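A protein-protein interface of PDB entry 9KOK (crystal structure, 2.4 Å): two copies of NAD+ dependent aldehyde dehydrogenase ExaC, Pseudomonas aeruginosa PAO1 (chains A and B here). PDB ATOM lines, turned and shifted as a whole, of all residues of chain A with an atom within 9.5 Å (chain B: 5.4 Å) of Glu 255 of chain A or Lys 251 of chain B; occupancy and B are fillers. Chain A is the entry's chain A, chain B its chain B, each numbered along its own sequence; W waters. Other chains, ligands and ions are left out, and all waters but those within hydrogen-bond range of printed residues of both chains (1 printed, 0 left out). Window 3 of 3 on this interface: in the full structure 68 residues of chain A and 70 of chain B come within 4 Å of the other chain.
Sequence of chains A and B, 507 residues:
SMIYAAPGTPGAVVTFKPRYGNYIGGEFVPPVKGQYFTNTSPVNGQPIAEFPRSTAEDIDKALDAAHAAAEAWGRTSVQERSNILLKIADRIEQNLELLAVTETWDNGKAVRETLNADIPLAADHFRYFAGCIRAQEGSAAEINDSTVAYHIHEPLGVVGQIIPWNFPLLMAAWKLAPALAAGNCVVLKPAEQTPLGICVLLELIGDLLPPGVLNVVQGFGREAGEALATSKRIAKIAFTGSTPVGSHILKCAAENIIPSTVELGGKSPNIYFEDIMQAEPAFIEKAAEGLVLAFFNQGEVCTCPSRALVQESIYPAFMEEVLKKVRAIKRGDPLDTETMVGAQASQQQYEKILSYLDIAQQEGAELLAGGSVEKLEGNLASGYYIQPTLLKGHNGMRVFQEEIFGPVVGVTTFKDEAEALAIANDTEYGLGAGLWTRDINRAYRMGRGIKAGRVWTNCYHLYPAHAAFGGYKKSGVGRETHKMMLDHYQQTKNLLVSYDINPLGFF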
ATOM      1  N   ALA A 229     -12.801  34.849  16.720  1.00  0.00           N
ATOM      2  CA  ALA A 229     -11.447  34.311  16.812  1.00  0.00           C
ATOM      3  C   ALA A 229     -11.202  33.193  15.799  1.00  0.00           C
ATOM      4  O   ALA A 229     -10.057  32.981  15.382  1.00  0.00           O
ATOM      5  CB  ALA A 229     -11.152  33.813  18.242  1.00  0.00           C
ATOM      6  N   THR A 230     -12.233  32.434  15.428  1.00  0.00           N
ATOM      7  CA  THR A 230     -12.076  31.373  14.432  1.00  0.00           C
ATOM      8  C   THR A 230     -12.380  31.846  13.016  1.00  0.00           C
ATOM      9  O   THR A 230     -12.259  31.059  12.071  1.00  0.00           O
ATOM     10  CB  THR A 230     -12.989  30.171  14.761  1.00  0.00           C
ATOM     11  OG1 THR A 230     -14.346  30.625  14.875  1.00  0.00           O
ATOM     12  CG2 THR A 230     -12.572  29.514  16.091  1.00  0.00           C
ATOM     13  N   SER A 231     -12.753  33.106  12.837  1.00  0.00           N
ATOM     14  CA  SER A 231     -13.190  33.544  11.523  1.00  0.00           C
ATOM     15  C   SER A 231     -12.070  33.427  10.499  1.00  0.00           C
ATOM     16  O   SER A 231     -10.907  33.756  10.765  1.00  0.00           O
ATOM     17  CB  SER A 231     -13.694  34.979  11.569  1.00  0.00           C
ATOM     18  OG  SER A 231     -13.887  35.414  10.242  1.00  0.00           O
ATOM     19  N   LYS A 232     -12.435  32.963   9.318  1.00  0.00           N
ATOM     20  CA  LYS A 232     -11.514  32.871   8.204  1.00  0.00           C
ATOM     21  C   LYS A 232     -11.452  34.158   7.397  1.00  0.00           C
ATOM     22  O   LYS A 232     -10.745  34.204   6.390  1.00  0.00           O
ATOM     23  CB  LYS A 232     -11.924  31.713   7.291  1.00  0.00           C
ATOM     24  CG  LYS A 232     -11.524  30.333   7.818  1.00  0.00           C
ATOM     25  CD  LYS A 232     -12.467  29.256   7.281  1.00  0.00           C
ATOM     26  CE  LYS A 232     -11.767  27.909   7.137  1.00  0.00           C
ATOM     27  NZ  LYS A 232     -10.754  27.621   8.208  1.00  0.00           N
ATOM     28  N   ILE A 237      -5.533  38.692  14.570  1.00  0.00           N
ATOM     29  CA  ILE A 237      -6.363  38.639  15.769  1.00  0.00           C
ATOM     30  C   ILE A 237      -5.566  39.221  16.922  1.00  0.00           C
ATOM     31  O   ILE A 237      -4.374  38.921  17.075  1.00  0.00           O
ATOM     32  CB  ILE A 237      -6.831  37.193  16.087  1.00  0.00           C
ATOM     33  CG1 ILE A 237      -7.753  37.186  17.308  1.00  0.00           C
ATOM     34  CG2 ILE A 237      -5.624  36.228  16.296  1.00  0.00           C
ATOM     35  CD1 ILE A 237      -9.121  37.721  17.030  1.00  0.00           C
ATOM     36  N   GLY A 246      -6.371  32.984  25.946  1.00  0.00           N
ATOM     37  CA  GLY A 246      -5.333  33.474  25.042  1.00  0.00           C
ATOM     38  C   GLY A 246      -4.651  32.357  24.270  1.00  0.00           C
ATOM     39  O   GLY A 246      -4.493  32.428  23.044  1.00  0.00           O
ATOM     40  N   SER A 247      -4.274  31.287  24.974  1.00  0.00           N
ATOM     41  CA  SER A 247      -3.711  30.123  24.299  1.00  0.00           C
ATOM     42  C   SER A 247      -4.663  29.606  23.228  1.00  0.00           C
ATOM     43  O   SER A 247      -4.234  29.272  22.118  1.00  0.00           O
ATOM     44  CB  SER A 247      -3.396  29.030  25.324  1.00  0.00           C
ATOM     45  OG  SER A 247      -2.739  27.940  24.716  1.00  0.00           O
ATOM     46  N   HIS A 248      -5.965  29.549  23.547  1.00  0.00           N
ATOM     47  CA  HIS A 248      -6.971  29.165  22.559  1.00  0.00           C
ATOM     48  C   HIS A 248      -6.981  30.116  21.361  1.00  0.00           C
ATOM     49  O   HIS A 248      -7.058  29.670  20.207  1.00  0.00           O
ATOM     50  CB  HIS A 248      -8.349  29.133  23.220  1.00  0.00           C
ATOM     51  CG  HIS A 248      -9.477  28.892  22.259  1.00  0.00           C
ATOM     52  ND1 HIS A 248      -9.676  27.678  21.628  1.00  0.00           N
ATOM     53  CD2 HIS A 248     -10.472  29.708  21.825  1.00  0.00           C
ATOM     54  CE1 HIS A 248     -10.734  27.761  20.840  1.00  0.00           C
ATOM     55  NE2 HIS A 248     -11.235  28.980  20.940  1.00  0.00           N
ATOM     56  N   ILE A 249      -6.917  31.429  21.621  1.00  0.00           N
ATOM     57  CA  ILE A 249      -6.830  32.422  20.548  1.00  0.00           C
ATOM     58  C   ILE A 249      -5.644  32.120  19.637  1.00  0.00           C
ATOM     59  O   ILE A 249      -5.768  32.122  18.406  1.00  0.00           O
ATOM     60  CB  ILE A 249      -6.713  33.838  21.143  1.00  0.00           C
ATOM     61  CG1 ILE A 249      -8.004  34.279  21.868  1.00  0.00           C
ATOM     62  CG2 ILE A 249      -6.231  34.831  20.080  1.00  0.00           C
ATOM     63  CD1 ILE A 249      -9.267  33.889  21.218  1.00  0.00           C
ATOM     64  N   LEU A 250      -4.476  31.848  20.233  1.00  0.00           N
ATOM     65  CA  LEU A 250      -3.296  31.547  19.431  1.00  0.00           C
ATOM     66  C   LEU A 250      -3.497  30.277  18.614  1.00  0.00           C
ATOM     67  O   LEU A 250      -3.002  30.171  17.486  1.00  0.00           O
ATOM     68  CB  LEU A 250      -2.052  31.431  20.327  1.00  0.00           C
ATOM     69  CG  LEU A 250      -1.520  32.685  21.052  1.00  0.00           C
ATOM     70  CD1 LEU A 250      -0.389  32.347  22.041  1.00  0.00           C
ATOM     71  CD2 LEU A 250      -1.053  33.742  20.058  1.00  0.00           C
ATOM     72  N   LYS A 251      -4.214  29.293  19.172  1.00  0.00           N
ATOM     73  CA  LYS A 251      -4.505  28.071  18.424  1.00  0.00           C
ATOM     74  C   LYS A 251      -5.436  28.359  17.248  1.00  0.00           C
ATOM     75  O   LYS A 251      -5.253  27.807  16.151  1.00  0.00           O
ATOM     76  CB  LYS A 251      -5.128  27.025  19.353  1.00  0.00           C
ATOM     77  CG  LYS A 251      -4.167  25.994  19.925  1.00  0.00           C
ATOM     78  CD  LYS A 251      -4.320  25.886  21.446  1.00  0.00           C
ATOM     79  CE  LYS A 251      -3.968  24.490  21.971  1.00  0.00           C
ATOM     80  NZ  LYS A 251      -4.443  24.284  23.380  1.00  0.00           N
ATOM     81  N   CYS A 252      -6.435  29.229  17.457  1.00  0.00           N
ATOM     82  CA  CYS A 252      -7.300  29.633  16.352  1.00  0.00           C
ATOM     83  C   CYS A 252      -6.502  30.331  15.258  1.00  0.00           C
ATOM     84  O   CYS A 252      -6.740  30.102  14.072  1.00  0.00           O
ATOM     85  CB  CYS A 252      -8.416  30.543  16.857  1.00  0.00           C
ATOM     86  SG  CYS A 252      -9.454  29.782  18.101  1.00  0.00           S
ATOM     87  N   ALA A 253      -5.554  31.193  15.645  1.00  0.00           N
ATOM     88  CA  ALA A 253      -4.720  31.879  14.668  1.00  0.00           C
ATOM     89  C   ALA A 253      -3.796  30.901  13.952  1.00  0.00           C
ATOM     90  O   ALA A 253      -3.585  31.011  12.737  1.00  0.00           O
ATOM     91  CB  ALA A 253      -3.900  32.973  15.363  1.00  0.00           C
ATOM     92  N   ALA A 254      -3.242  29.938  14.694  1.00  0.00           N
ATOM     93  CA  ALA A 254      -2.421  28.889  14.097  1.00  0.00           C
ATOM     94  C   ALA A 254      -3.171  28.150  12.998  1.00  0.00           C
ATOM     95  O   ALA A 254      -2.602  27.854  11.947  1.00  0.00           O
ATOM     96  CB  ALA A 254      -1.969  27.898  15.172  1.00  0.00           C
ATOM     97  N   GLU A 255      -4.439  27.813  13.237  1.00  0.00           N
ATOM     98  CA  GLU A 255      -5.205  27.059  12.248  1.00  0.00           C
ATOM     99  C   GLU A 255      -5.366  27.842  10.947  1.00  0.00           C
ATOM    100  O   GLU A 255      -5.318  27.256   9.863  1.00  0.00           O
ATOM    101  CB  GLU A 255      -6.568  26.666  12.831  1.00  0.00           C
ATOM    102  CG  GLU A 255      -7.645  26.288  11.809  1.00  0.00           C
ATOM    103  CD  GLU A 255      -7.480  24.869  11.271  1.00  0.00           C
ATOM    104  OE1 GLU A 255      -6.737  24.083  11.908  1.00  0.00           O
ATOM    105  OE2 GLU A 255      -8.073  24.551  10.206  1.00  0.00           O
ATOM    106  N   ASN A 256      -5.561  29.158  11.028  1.00  0.00           N
ATOM    107  CA  ASN A 256      -5.792  29.977   9.845  1.00  0.00           C
ATOM    108  C   ASN A 256      -4.522  30.632   9.331  1.00  0.00           C
ATOM    109  O   ASN A 256      -4.581  31.347   8.326  1.00  0.00           O
ATOM    110  CB  ASN A 256      -6.839  31.063  10.131  1.00  0.00           C
ATOM    111  CG  ASN A 256      -8.247  30.502  10.289  1.00  0.00           C
ATOM    112  OD1 ASN A 256      -8.658  29.587   9.562  1.00  0.00           O
ATOM    113  ND2 ASN A 256      -8.993  31.050  11.236  1.00  0.00           N
ATOM    114  N   ILE A 257      -3.384  30.421  10.002  1.00  0.00           N
ATOM    115  CA  ILE A 257      -2.103  31.024   9.629  1.00  0.00           C
ATOM    116  C   ILE A 257      -2.213  32.548   9.532  1.00  0.00           C
ATOM    117  O   ILE A 257      -1.838  33.157   8.523  1.00  0.00           O
ATOM    118  CB  ILE A 257      -1.591  30.383   8.326  1.00  0.00           C
ATOM    119  CG1 ILE A 257      -1.779  28.863   8.442  1.00  0.00           C
ATOM    120  CG2 ILE A 257      -0.119  30.714   8.074  1.00  0.00           C
ATOM    121  CD1 ILE A 257      -1.166  28.072   7.352  1.00  0.00           C
ATOM    122  N   ILE A 258      -2.714  33.176  10.594  1.00  0.00           N
ATOM    123  CA  ILE A 258      -2.749  34.626  10.654  1.00  0.00           C
ATOM    124  C   ILE A 258      -1.911  35.071  11.847  1.00  0.00           C
ATOM    125  O   ILE A 258      -1.810  34.340  12.845  1.00  0.00           O
ATOM    126  CB  ILE A 258      -4.184  35.163  10.752  1.00  0.00           C
ATOM    127  CG1 ILE A 258      -4.890  34.597  11.988  1.00  0.00           C
ATOM    128  CG2 ILE A 258      -4.962  34.929   9.442  1.00  0.00           C
ATOM    129  CD1 ILE A 258      -6.123  35.409  12.368  1.00  0.00           C
ATOM    130  N   PRO A 259      -1.292  36.251  11.777  1.00  0.00           N
ATOM    131  CA  PRO A 259      -0.557  36.776  12.936  1.00  0.00           C
ATOM    132  C   PRO A 259      -1.471  37.055  14.119  1.00  0.00           C
ATOM    133  O   PRO A 259      -2.652  37.371  13.968  1.00  0.00           O
ATOM    134  CB  PRO A 259       0.058  38.082  12.421  1.00  0.00           C
ATOM    135  CG  PRO A 259      -0.403  38.257  11.023  1.00  0.00           C
ATOM    136  CD  PRO A 259      -1.351  37.193  10.645  1.00  0.00           C
ATOM    137  N   SER A 260      -0.883  37.010  15.307  1.00  0.00           N
ATOM    138  CA  SER A 260      -1.643  37.169  16.540  1.00  0.00           C
ATOM    139  C   SER A 260      -0.785  37.882  17.566  1.00  0.00           C
ATOM    140  O   SER A 260       0.431  37.700  17.603  1.00  0.00           O
ATOM    141  CB  SER A 260      -2.073  35.812  17.113  1.00  0.00           C
ATOM    142  OG  SER A 260      -0.930  34.966  17.197  1.00  0.00           O
ATOM    143  N   GLY B 246       3.747  23.366   9.298  1.00  0.00           N
ATOM    144  CA  GLY B 246       3.844  24.733   9.779  1.00  0.00           C
ATOM    145  C   GLY B 246       2.663  25.142  10.636  1.00  0.00           C
ATOM    146  O   GLY B 246       2.833  25.778  11.679  1.00  0.00           O
ATOM    147  N   SER B 247       1.448  24.809  10.197  1.00  0.00           N
ATOM    148  CA  SER B 247       0.280  25.050  11.037  1.00  0.00           C
ATOM    149  C   SER B 247       0.395  24.326  12.377  1.00  0.00           C
ATOM    150  O   SER B 247       0.093  24.904  13.428  1.00  0.00           O
ATOM    151  CB  SER B 247      -0.985  24.617  10.310  1.00  0.00           C
ATOM    152  OG  SER B 247      -2.088  25.317  10.866  1.00  0.00           O
ATOM    153  N   HIS B 248       0.828  23.058  12.353  1.00  0.00           N
ATOM    154  CA  HIS B 248       1.093  22.303  13.581  1.00  0.00           C
ATOM    155  C   HIS B 248       2.165  22.983  14.438  1.00  0.00           C
ATOM    156  O   HIS B 248       2.028  23.074  15.665  1.00  0.00           O
ATOM    157  CB  HIS B 248       1.485  20.865  13.203  1.00  0.00           C
ATOM    158  CG  HIS B 248       2.117  20.075  14.307  1.00  0.00           C
ATOM    159  ND1 HIS B 248       1.397  19.568  15.371  1.00  0.00           N
ATOM    160  CD2 HIS B 248       3.396  19.662  14.487  1.00  0.00           C
ATOM    161  CE1 HIS B 248       2.212  18.907  16.174  1.00  0.00           C
ATOM    162  NE2 HIS B 248       3.428  18.942  15.658  1.00  0.00           N
ATOM    163  N   ILE B 249       3.236  23.480  13.813  1.00  0.00           N
ATOM    164  CA  ILE B 249       4.241  24.248  14.553  1.00  0.00           C
ATOM    165  C   ILE B 249       3.591  25.438  15.266  1.00  0.00           C
ATOM    166  O   ILE B 249       3.853  25.704  16.447  1.00  0.00           O
ATOM    167  CB  ILE B 249       5.358  24.716  13.606  1.00  0.00           C
ATOM    168  CG1 ILE B 249       6.114  23.523  12.984  1.00  0.00           C
ATOM    169  CG2 ILE B 249       6.295  25.653  14.330  1.00  0.00           C
ATOM    170  CD1 ILE B 249       6.989  22.801  13.929  1.00  0.00           C
ATOM    171  N   LEU B 250       2.739  26.181  14.548  1.00  0.00           N
ATOM    172  CA  LEU B 250       2.082  27.334  15.147  1.00  0.00           C
ATOM    173  C   LEU B 250       1.195  26.906  16.313  1.00  0.00           C
ATOM    174  O   LEU B 250       1.110  27.612  17.325  1.00  0.00           O
ATOM    175  CB  LEU B 250       1.272  28.089  14.085  1.00  0.00           C
ATOM    176  CG  LEU B 250       1.965  28.911  12.997  1.00  0.00           C
ATOM    177  CD1 LEU B 250       0.938  29.482  12.008  1.00  0.00           C
ATOM    178  CD2 LEU B 250       2.812  30.042  13.619  1.00  0.00           C
ATOM    179  N   LYS B 251       0.554  25.732  16.204  1.00  0.00           N
ATOM    180  CA  LYS B 251      -0.259  25.218  17.304  1.00  0.00           C
ATOM    181  C   LYS B 251       0.606  24.827  18.499  1.00  0.00           C
ATOM    182  O   LYS B 251       0.212  25.044  19.649  1.00  0.00           O
ATOM    183  CB  LYS B 251      -1.101  24.020  16.837  1.00  0.00           C
ATOM    184  CG  LYS B 251      -2.347  24.421  16.044  1.00  0.00           C
ATOM    185  CD  LYS B 251      -3.239  23.231  15.679  1.00  0.00           C
ATOM    186  CE  LYS B 251      -3.875  23.374  14.276  1.00  0.00           C
ATOM    187  NZ  LYS B 251      -3.221  22.478  13.247  1.00  0.00           N
ATOM    188  N   CYS B 252       1.778  24.234  18.248  1.00  0.00           N
ATOM    189  CA  CYS B 252       2.701  23.917  19.333  1.00  0.00           C
ATOM    190  C   CYS B 252       3.145  25.173  20.069  1.00  0.00           C
ATOM    191  O   CYS B 252       3.240  25.184  21.304  1.00  0.00           O
ATOM    192  CB  CYS B 252       3.919  23.181  18.781  1.00  0.00           C
ATOM    193  SG  CYS B 252       3.555  21.518  18.168  1.00  0.00           S
ATOM    194  N   ALA B 253       3.434  26.240  19.327  1.00  0.00           N
ATOM    195  CA  ALA B 253       3.823  27.483  19.971  1.00  0.00           C
ATOM    196  C   ALA B 253       2.652  28.079  20.737  1.00  0.00           C
ATOM    197  O   ALA B 253       2.835  28.640  21.825  1.00  0.00           O
ATOM    198  CB  ALA B 253       4.347  28.470  18.923  1.00  0.00           C
ATOM    199  N   ALA B 254       1.441  27.980  20.174  1.00  0.00           N
ATOM    200  CA  ALA B 254       0.246  28.472  20.855  1.00  0.00           C
ATOM    201  C   ALA B 254       0.104  27.828  22.222  1.00  0.00           C
ATOM    202  O   ALA B 254      -0.152  28.512  23.221  1.00  0.00           O
ATOM    203  CB  ALA B 254      -1.000  28.193  20.011  1.00  0.00           C
ATOM    204  N   GLU B 255       0.301  26.509  22.284  1.00  0.00           N
ATOM    205  CA  GLU B 255       0.153  25.796  23.543  1.00  0.00           C
ATOM    206  C   GLU B 255       1.146  26.310  24.576  1.00  0.00           C
ATOM    207  O   GLU B 255       0.807  26.454  25.759  1.00  0.00           O
ATOM    208  CB  GLU B 255       0.331  24.294  23.311  1.00  0.00           C
ATOM    209  CG  GLU B 255       0.428  23.453  24.585  1.00  0.00           C
ATOM    210  CD  GLU B 255      -0.892  23.376  25.359  1.00  0.00           C
ATOM    211  OE1 GLU B 255      -0.853  23.374  26.616  1.00  0.00           O
ATOM    212  OE2 GLU B 255      -1.965  23.333  24.710  1.00  0.00           O
ATOM    213  N   ASN B 256       2.365  26.635  24.140  1.00  0.00           N
ATOM    214  CA  ASN B 256       3.428  27.030  25.050  1.00  0.00           C
ATOM    215  C   ASN B 256       3.572  28.542  25.194  1.00  0.00           C
ATOM    216  O   ASN B 256       4.432  28.987  25.956  1.00  0.00           O
ATOM    217  CB  ASN B 256       4.740  26.388  24.597  1.00  0.00           C
ATOM    218  CG  ASN B 256       4.752  24.886  24.851  1.00  0.00           C
ATOM    219  OD1 ASN B 256       4.146  24.432  25.806  1.00  0.00           O
ATOM    220  ND2 ASN B 256       5.439  24.118  24.007  1.00  0.00           N
HETATM  221  O   HOH W   1      -1.521  26.934  27.671  1.00  0.00           O
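The side-chain hydroxyl (OG) of Ser 247 of chain A sits at hydrogen-bond distance from the backbone carbonyl oxygen (O) of Ala 254 of chain B (3.0 Å). The side-chain carboxylate (OE2) of Glu 255 of chain B lies within salt-bridge range of the side-chain amino group (NZ) of Lys 251 of chain A (3.0 Å). OG of Ser 247 of chain B sits at hydrogen-bond distance from O of Ala 254 of chain A, at 2.8 Å.
CA of Glu 255 of chain B touches OG of Ser 247 of chain A, 3.8 Å away. Leu 250 of chain A touches Ala 254 of chain B (CB to CB, 3.4 Å). CB of Ala 254 of chain B touches N of Lys 251 of chain A, 3.5 Å away. Leu 250 of chain B touches Ala 254 of chain A (CB to CB, 3.4 Å). N of Lys 251 of chain B touches CB of Ala 254 of chain A, at 3.5 Å. OG of Ser 247 of chain B touches CA of Glu 255 of chain A, at 3.8 Å. Glu 255 of chain A touches Lys 251 of chain B (OE1 to CE, 3.8 Å).
Of the printed residues of chain B, Lys 251 of chain A touches Ala 254 (3.5 Å) and Glu 255 (3.0 Å). Of the printed residues of chain B, Ala 254 of chain A touches Ser 247 (2.8 Å), Leu 250 (3.4 Å) and Lys 251 (3.5 Å). Glu 255 of chain A touches two residues of chain B. No residue of chain A comes within 4 Å of Cys 252 of chain B. No residue of chain A comes within 4 Å of Ala 253 of chain B. The nearest printed residue of chain B that does not touch Leu 250 of chain A is Leu 250 of chain B (4.8 Å).
Of the 20 printed residues of chain A, 5 touch a printed residue of chain B. Hydrophobic or aromatic side chains of chain A that line the printed part of chain B: Leu 250 and Ala 254. Of the 11 printed residues of chain B, 5 touch a printed residue of chain A. Hydrophobic or aromatic side chains of chain B that line the printed part of chain A: Leu 250 and Ala 254. Among the printed residues, Asp or Glu carboxylates within 4 Å of a Lys or Arg side-chain nitrogen of the other chain: Lys 251 of chain A with Glu 255 of chain B.
Ser 247 of chain A touches Ala 254 of chain B, and with the chains exchanged Ala 254 of chain A touches Ser 247 of chain B. Ser 247 of chain A touches Glu 255 of chain B, and with the chains exchanged Glu 255 of chain A touches Ser 247 of chain B. Leu 250 of chain A touches Ala 254 of chain B, and with the chains exchanged Ala 254 of chain A touches Leu 250 of chain B. Lys 251 of chain A touches Glu 255 of chain B, and with the chains exchanged Glu 255 of chain A touches Lys 251 of chain B. Positions printed for both chains: 246, 247, 248, 249, 250, 251, 252, 253, 254, 255 and 256. Of the 10 pairs that touch across the chains among the printed residues, 10 have their exchanged pair printed and touching as well.
Water W1 bridges O of Glu 255 of chain B (3.1 Å) and OG of Ser 247 of chain A (3.4 Å).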
